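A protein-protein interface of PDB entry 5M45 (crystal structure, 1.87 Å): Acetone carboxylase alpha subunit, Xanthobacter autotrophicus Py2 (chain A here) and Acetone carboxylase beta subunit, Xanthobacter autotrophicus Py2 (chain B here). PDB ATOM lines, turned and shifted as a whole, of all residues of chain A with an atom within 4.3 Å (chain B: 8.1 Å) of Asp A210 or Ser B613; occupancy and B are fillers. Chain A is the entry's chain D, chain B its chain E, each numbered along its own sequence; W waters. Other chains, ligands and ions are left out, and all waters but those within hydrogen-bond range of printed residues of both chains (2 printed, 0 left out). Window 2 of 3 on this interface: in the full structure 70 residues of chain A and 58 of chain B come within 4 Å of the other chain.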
ATOM      1  N   LYS A 136     -23.170  -2.497   0.262  1.00  0.00           N
ATOM      2  CA  LYS A 136     -23.160  -2.785   1.712  1.00  0.00           C
ATOM      3  C   LYS A 136     -22.012  -3.741   2.188  1.00  0.00           C
ATOM      4  O   LYS A 136     -21.996  -4.158   3.343  1.00  0.00           O
ATOM      5  CB  LYS A 136     -24.509  -3.259   2.205  1.00  0.00           C
ATOM      6  CG  LYS A 136     -25.660  -2.319   1.891  1.00  0.00           C
ATOM      7  CD  LYS A 136     -26.892  -2.850   2.690  1.00  0.00           C
ATOM      8  CE  LYS A 136     -28.229  -2.522   2.065  1.00  0.00           C
ATOM      9  NZ  LYS A 136     -28.316  -1.069   1.823  1.00  0.00           N
ATOM     10  N   ILE A 138     -18.172  -4.507   3.404  1.00  0.00           N
ATOM     11  CA  ILE A 138     -17.131  -3.821   4.187  1.00  0.00           C
ATOM     12  C   ILE A 138     -15.775  -4.491   3.933  1.00  0.00           C
ATOM     13  O   ILE A 138     -15.632  -5.701   4.155  1.00  0.00           O
ATOM     14  CB  ILE A 138     -17.436  -3.871   5.702  1.00  0.00           C
ATOM     15  CG1 ILE A 138     -18.879  -3.385   5.987  1.00  0.00           C
ATOM     16  CG2 ILE A 138     -16.386  -3.090   6.499  1.00  0.00           C
ATOM     17  CD1 ILE A 138     -19.304  -3.505   7.444  1.00  0.00           C
ATOM     18  N   ALA A 208     -20.661  -7.903   5.111  1.00  0.00           N
ATOM     19  CA  ALA A 208     -21.651  -7.771   4.041  1.00  0.00           C
ATOM     20  C   ALA A 208     -22.999  -7.420   4.677  1.00  0.00           C
ATOM     21  O   ALA A 208     -23.217  -7.670   5.855  1.00  0.00           O
ATOM     22  CB  ALA A 208     -21.731  -9.061   3.207  1.00  0.00           C
ATOM     23  N   ASN A 209     -23.877  -6.790   3.891  1.00  0.00           N
ATOM     24  CA  ASN A 209     -25.134  -6.253   4.390  1.00  0.00           C
ATOM     25  C   ASN A 209     -24.899  -5.396   5.660  1.00  0.00           C
ATOM     26  O   ASN A 209     -25.629  -5.492   6.658  1.00  0.00           O
ATOM     27  CB  ASN A 209     -26.113  -7.433   4.651  1.00  0.00           C
ATOM     28  CG  ASN A 209     -27.540  -6.961   4.816  1.00  0.00           C
ATOM     29  OD1 ASN A 209     -27.989  -5.988   4.169  1.00  0.00           O
ATOM     30  ND2 ASN A 209     -28.286  -7.638   5.702  1.00  0.00           N
ATOM     31  N   ASP A 210     -23.843  -4.594   5.634  1.00  0.00           N
ATOM     32  CA  ASP A 210     -23.501  -3.658   6.720  1.00  0.00           C
ATOM     33  C   ASP A 210     -23.186  -4.343   8.062  1.00  0.00           C
ATOM     34  O   ASP A 210     -23.218  -3.696   9.103  1.00  0.00           O
ATOM     35  CB  ASP A 210     -24.612  -2.558   6.885  1.00  0.00           C
ATOM     36  CG  ASP A 210     -24.584  -1.498   5.777  1.00  0.00           C
ATOM     37  OD1 ASP A 210     -23.665  -1.497   4.889  1.00  0.00           O
ATOM     38  OD2 ASP A 210     -25.477  -0.615   5.785  1.00  0.00           O
ATOM     39  N   THR A 211     -22.838  -5.627   8.015  1.00  0.00           N
ATOM     40  CA  THR A 211     -22.679  -6.449   9.216  1.00  0.00           C
ATOM     41  C   THR A 211     -21.314  -7.146   9.183  1.00  0.00           C
ATOM     42  O   THR A 211     -20.993  -7.828   8.203  1.00  0.00           O
ATOM     43  CB  THR A 211     -23.779  -7.514   9.297  1.00  0.00           C
ATOM     44  OG1 THR A 211     -25.048  -6.865   9.189  1.00  0.00           O
ATOM     45  CG2 THR A 211     -23.750  -8.275  10.610  1.00  0.00           C
ATOM     46  N   ARG A 235     -15.210   0.456  15.232  1.00  0.00           N
ATOM     47  CA  ARG A 235     -16.521   1.113  15.198  1.00  0.00           C
ATOM     48  C   ARG A 235     -16.425   2.573  14.752  1.00  0.00           C
ATOM     49  O   ARG A 235     -17.290   3.033  13.999  1.00  0.00           O
ATOM     50  CB  ARG A 235     -17.257   0.991  16.549  1.00  0.00           C
ATOM     51  CG  ARG A 235     -17.501  -0.405  17.061  1.00  0.00           C
ATOM     52  CD  ARG A 235     -18.407  -1.204  16.131  1.00  0.00           C
ATOM     53  NE  ARG A 235     -18.688  -2.546  16.635  1.00  0.00           N
ATOM     54  CZ  ARG A 235     -19.489  -3.418  16.010  1.00  0.00           C
ATOM     55  NH1 ARG A 235     -19.687  -4.621  16.576  1.00  0.00           N
ATOM     56  NH2 ARG A 235     -20.111  -3.127  14.858  1.00  0.00           N
ATOM     57  N   ILE A 238     -16.054   2.504  10.811  1.00  0.00           N
ATOM     58  CA  ILE A 238     -17.287   2.136  10.123  1.00  0.00           C
ATOM     59  C   ILE A 238     -18.343   3.264  10.242  1.00  0.00           C
ATOM     60  O   ILE A 238     -19.076   3.519   9.277  1.00  0.00           O
ATOM     61  CB  ILE A 238     -17.843   0.779  10.584  1.00  0.00           C
ATOM     62  CG1 ILE A 238     -18.843   0.201   9.570  1.00  0.00           C
ATOM     63  CG2 ILE A 238     -18.652   0.821  11.848  1.00  0.00           C
ATOM     64  CD1 ILE A 238     -18.301   0.046   8.134  1.00  0.00           C
ATOM     65  N   HIS A 242     -20.002   5.147   6.922  1.00  0.00           N
ATOM     66  CA  HIS A 242     -21.457   5.114   6.712  1.00  0.00           C
ATOM     67  C   HIS A 242     -22.124   6.504   6.775  1.00  0.00           C
ATOM     68  O   HIS A 242     -23.066   6.751   6.020  1.00  0.00           O
ATOM     69  CB  HIS A 242     -22.161   4.070   7.619  1.00  0.00           C
ATOM     70  CG  HIS A 242     -21.909   2.655   7.192  1.00  0.00           C
ATOM     71  ND1 HIS A 242     -22.379   1.562   7.899  1.00  0.00           N
ATOM     72  CD2 HIS A 242     -21.254   2.152   6.112  1.00  0.00           C
ATOM     73  CE1 HIS A 242     -22.009   0.456   7.272  1.00  0.00           C
ATOM     74  NE2 HIS A 242     -21.345   0.793   6.176  1.00  0.00           N
ATOM     75  N   ARG A 245     -21.247   7.831   3.233  1.00  0.00           N
ATOM     76  CA  ARG A 245     -22.090   7.138   2.239  1.00  0.00           C
ATOM     77  C   ARG A 245     -23.511   7.709   2.217  1.00  0.00           C
ATOM     78  O   ARG A 245     -24.056   8.005   1.141  1.00  0.00           O
ATOM     79  CB  ARG A 245     -22.139   5.628   2.483  1.00  0.00           C
ATOM     80  CG  ARG A 245     -22.888   4.834   1.405  1.00  0.00           C
ATOM     81  CD  ARG A 245     -22.996   3.363   1.744  1.00  0.00           C
ATOM     82  NE  ARG A 245     -23.751   3.160   2.980  1.00  0.00           N
ATOM     83  CZ  ARG A 245     -23.876   2.009   3.636  1.00  0.00           C
ATOM     84  NH1 ARG A 245     -23.306   0.887   3.191  1.00  0.00           N
ATOM     85  NH2 ARG A 245     -24.576   1.977   4.754  1.00  0.00           N
ATOM     86  N   TYR B 606     -27.720   6.343  19.719  1.00  0.00           N
ATOM     87  CA  TYR B 606     -26.336   6.173  19.252  1.00  0.00           C
ATOM     88  C   TYR B 606     -26.326   5.857  17.778  1.00  0.00           C
ATOM     89  O   TYR B 606     -25.468   6.345  17.038  1.00  0.00           O
ATOM     90  CB  TYR B 606     -25.662   5.066  20.039  1.00  0.00           C
ATOM     91  CG  TYR B 606     -24.151   4.946  20.021  1.00  0.00           C
ATOM     92  CD1 TYR B 606     -23.503   4.199  19.034  1.00  0.00           C
ATOM     93  CD2 TYR B 606     -23.380   5.508  21.033  1.00  0.00           C
ATOM     94  CE1 TYR B 606     -22.130   4.032  19.040  1.00  0.00           C
ATOM     95  CE2 TYR B 606     -21.971   5.362  21.072  1.00  0.00           C
ATOM     96  CZ  TYR B 606     -21.340   4.624  20.067  1.00  0.00           C
ATOM     97  OH  TYR B 606     -19.987   4.399  20.106  1.00  0.00           O
ATOM     98  N   GLY B 607     -27.279   5.053  17.330  1.00  0.00           N
ATOM     99  CA  GLY B 607     -27.441   4.753  15.897  1.00  0.00           C
ATOM    100  C   GLY B 607     -27.725   5.964  15.022  1.00  0.00           C
ATOM    101  O   GLY B 607     -27.219   6.062  13.895  1.00  0.00           O
ATOM    102  N   TYR B 610     -24.443   8.539  15.208  1.00  0.00           N
ATOM    103  CA  TYR B 610     -23.290   7.993  14.519  1.00  0.00           C
ATOM    104  C   TYR B 610     -23.792   7.148  13.332  1.00  0.00           C
ATOM    105  O   TYR B 610     -24.092   7.703  12.261  1.00  0.00           O
ATOM    106  CB  TYR B 610     -22.420   7.201  15.519  1.00  0.00           C
ATOM    107  CG  TYR B 610     -21.882   8.034  16.664  1.00  0.00           C
ATOM    108  CD1 TYR B 610     -21.017   9.108  16.432  1.00  0.00           C
ATOM    109  CD2 TYR B 610     -22.178   7.726  17.985  1.00  0.00           C
ATOM    110  CE1 TYR B 610     -20.513   9.877  17.498  1.00  0.00           C
ATOM    111  CE2 TYR B 610     -21.681   8.504  19.033  1.00  0.00           C
ATOM    112  CZ  TYR B 610     -20.847   9.587  18.768  1.00  0.00           C
ATOM    113  OH  TYR B 610     -20.380  10.348  19.826  1.00  0.00           O
ATOM    114  N   ALA B 611     -23.910   5.832  13.496  1.00  0.00           N
ATOM    115  CA  ALA B 611     -24.544   4.950  12.496  1.00  0.00           C
ATOM    116  C   ALA B 611     -24.961   3.651  13.164  1.00  0.00           C
ATOM    117  O   ALA B 611     -24.402   3.299  14.205  1.00  0.00           O
ATOM    118  CB  ALA B 611     -23.581   4.658  11.349  1.00  0.00           C
ATOM    119  N   ALA B 612     -25.922   2.921  12.569  1.00  0.00           N
ATOM    120  CA  ALA B 612     -26.379   1.635  13.148  1.00  0.00           C
ATOM    121  C   ALA B 612     -25.221   0.652  13.350  1.00  0.00           C
ATOM    122  O   ALA B 612     -25.158  -0.039  14.394  1.00  0.00           O
ATOM    123  CB  ALA B 612     -27.439   1.001  12.270  1.00  0.00           C
ATOM    124  N   SER B 613     -24.309   0.603  12.368  1.00  0.00           N
ATOM    125  CA  SER B 613     -23.166  -0.308  12.432  1.00  0.00           C
ATOM    126  C   SER B 613     -22.093   0.044  13.439  1.00  0.00           C
ATOM    127  O   SER B 613     -21.209  -0.754  13.687  1.00  0.00           O
ATOM    128  CB  SER B 613     -22.540  -0.429  11.039  1.00  0.00           C
ATOM    129  OG  SER B 613     -23.477  -1.130  10.189  1.00  0.00           O
ATOM    130  N   ALA B 614     -22.169   1.226  14.028  1.00  0.00           N
ATOM    131  CA  ALA B 614     -21.264   1.632  15.087  1.00  0.00           C
ATOM    132  C   ALA B 614     -21.607   1.111  16.469  1.00  0.00           C
ATOM    133  O   ALA B 614     -20.731   1.164  17.382  1.00  0.00           O
ATOM    134  CB  ALA B 614     -21.181   3.145  15.137  1.00  0.00           C
ATOM    135  N   ARG B 615     -22.832   0.623  16.657  1.00  0.00           N
ATOM    136  CA  ARG B 615     -23.238   0.140  17.986  1.00  0.00           C
ATOM    137  C   ARG B 615     -22.377  -1.070  18.414  1.00  0.00           C
ATOM    138  O   ARG B 615     -22.100  -1.928  17.578  1.00  0.00           O
ATOM    139  CB  ARG B 615     -24.686  -0.299  18.001  1.00  0.00           C
ATOM    140  CG  ARG B 615     -25.685   0.794  17.782  1.00  0.00           C
ATOM    141  CD  ARG B 615     -27.066   0.194  17.937  1.00  0.00           C
ATOM    142  NE  ARG B 615     -28.037   1.003  17.266  1.00  0.00           N
ATOM    143  CZ  ARG B 615     -28.763   0.663  16.217  1.00  0.00           C
ATOM    144  NH1 ARG B 615     -28.661  -0.541  15.648  1.00  0.00           N
ATOM    145  NH2 ARG B 615     -29.614   1.527  15.701  1.00  0.00           N
ATOM    146  N   SER B 616     -21.968  -1.077  19.699  1.00  0.00           N
ATOM    147  CA  SER B 616     -21.108  -2.109  20.280  1.00  0.00           C
ATOM    148  C   SER B 616     -21.645  -2.652  21.629  1.00  0.00           C
ATOM    149  O   SER B 616     -20.941  -2.599  22.640  1.00  0.00           O
ATOM    150  CB  SER B 616     -19.682  -1.556  20.473  1.00  0.00           C
ATOM    151  OG  SER B 616     -19.673  -0.393  21.301  1.00  0.00           O
ATOM    152  N   PRO B 617     -22.887  -3.189  21.633  1.00  0.00           N
ATOM    153  CA  PRO B 617     -23.525  -3.718  22.872  1.00  0.00           C
ATOM    154  C   PRO B 617     -22.727  -4.792  23.599  1.00  0.00           C
ATOM    155  O   PRO B 617     -22.843  -4.888  24.831  1.00  0.00           O
ATOM    156  CB  PRO B 617     -24.877  -4.271  22.385  1.00  0.00           C
ATOM    157  CG  PRO B 617     -24.683  -4.527  20.929  1.00  0.00           C
ATOM    158  CD  PRO B 617     -23.734  -3.459  20.447  1.00  0.00           C
ATOM    159  N   GLU B 618     -21.908  -5.556  22.858  1.00  0.00           N
ATOM    160  CA  GLU B 618     -21.040  -6.570  23.462  1.00  0.00           C
ATOM    161  C   GLU B 618     -20.071  -6.020  24.530  1.00  0.00           C
ATOM    162  O   GLU B 618     -19.585  -6.791  25.355  1.00  0.00           O
ATOM    163  CB  GLU B 618     -20.273  -7.362  22.388  1.00  0.00           C
ATOM    164  CG  GLU B 618     -19.212  -6.598  21.570  1.00  0.00           C
ATOM    165  CD  GLU B 618     -19.746  -5.880  20.311  1.00  0.00           C
ATOM    166  OE1 GLU B 618     -20.951  -5.491  20.243  1.00  0.00           O
ATOM    167  OE2 GLU B 618     -18.952  -5.612  19.396  1.00  0.00           O
HETATM  168  O   HOH W   1     -24.698   1.774   9.518  1.00  0.00           O
HETATM  169  O   HOH W   2     -17.120  -3.698  18.778  1.00  0.00           O
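The side-chain hydroxyl (OG) of Ser B613 sits at hydrogen-bond distance from the backbone carbonyl oxygen (O) of Asp A210, at 2.8 Å. The backbone carbonyl oxygen (O) of Ser B613 sits at hydrogen-bond distance from the guanidinium group (NH2) of Arg A235 (2.9 Å). The guanidinium group (NH1) of Arg A235 is in salt-bridge range of the side-chain carboxylate (OE2) of Glu B618 (3.1 Å).
The backbone carbonyl oxygen (O) of Lys A136 sits at hydrogen-bond distance from the backbone NH (N) of Asp A210 (3.0 Å). The side-chain carboxylate (OD2) of Asp A210 is in salt-bridge range of the guanidinium group (NH2) of Arg A245, at 2.9 Å.
Ala B614 touches Arg A235 (O to CD, 3.5 Å). O of Arg B615 touches CZ of Arg A235, 3.4 Å away. Ile A238 touches Ser B613 (CG2 to O, 3.5 Å). Ser B613 touches His A242 (OG to CE1, 3.6 Å).
Asp A210 touches one residue of chain B. Ser B613 touches four residues of chain A. Printed residues of chain A within 4 Å of Arg B615: Arg A235 (3.4 Å). Of the printed residues of chain B, His A242 touches Ser B613 (3.6 Å). Of the printed residues of chain A, Glu B618 touches Arg A235 (3.1 Å). The nearest residue of chain B that does not touch Asp A210 is Ala B612 (6.4 Å). The nearest printed residue of chain A that does not touch Ser B613 is Thr A211 (5.0 Å). The nearest printed residue of chain A that does not touch Glu B618 is Ile A238 (9.9 Å).
Of the 11 printed residues of chain B, 4 touch a printed residue of chain A. Printed residues of chain B that touch a printed residue of chain A: Ser B613, Ala B614, Arg B615 and Glu B618.
Water W2 lies within hydrogen-bond range of OE2 of Glu B618 (2.7 Å) and NE of Arg A235 (2.9 Å). Water W1 lies within hydrogen-bond range of a ring nitrogen (ND1) of His A242 (2.8 Å), the backbone NH (N) of Ser B613 (3.1 Å) and the backbone NH (N) of Ala B612 (3.5 Å).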
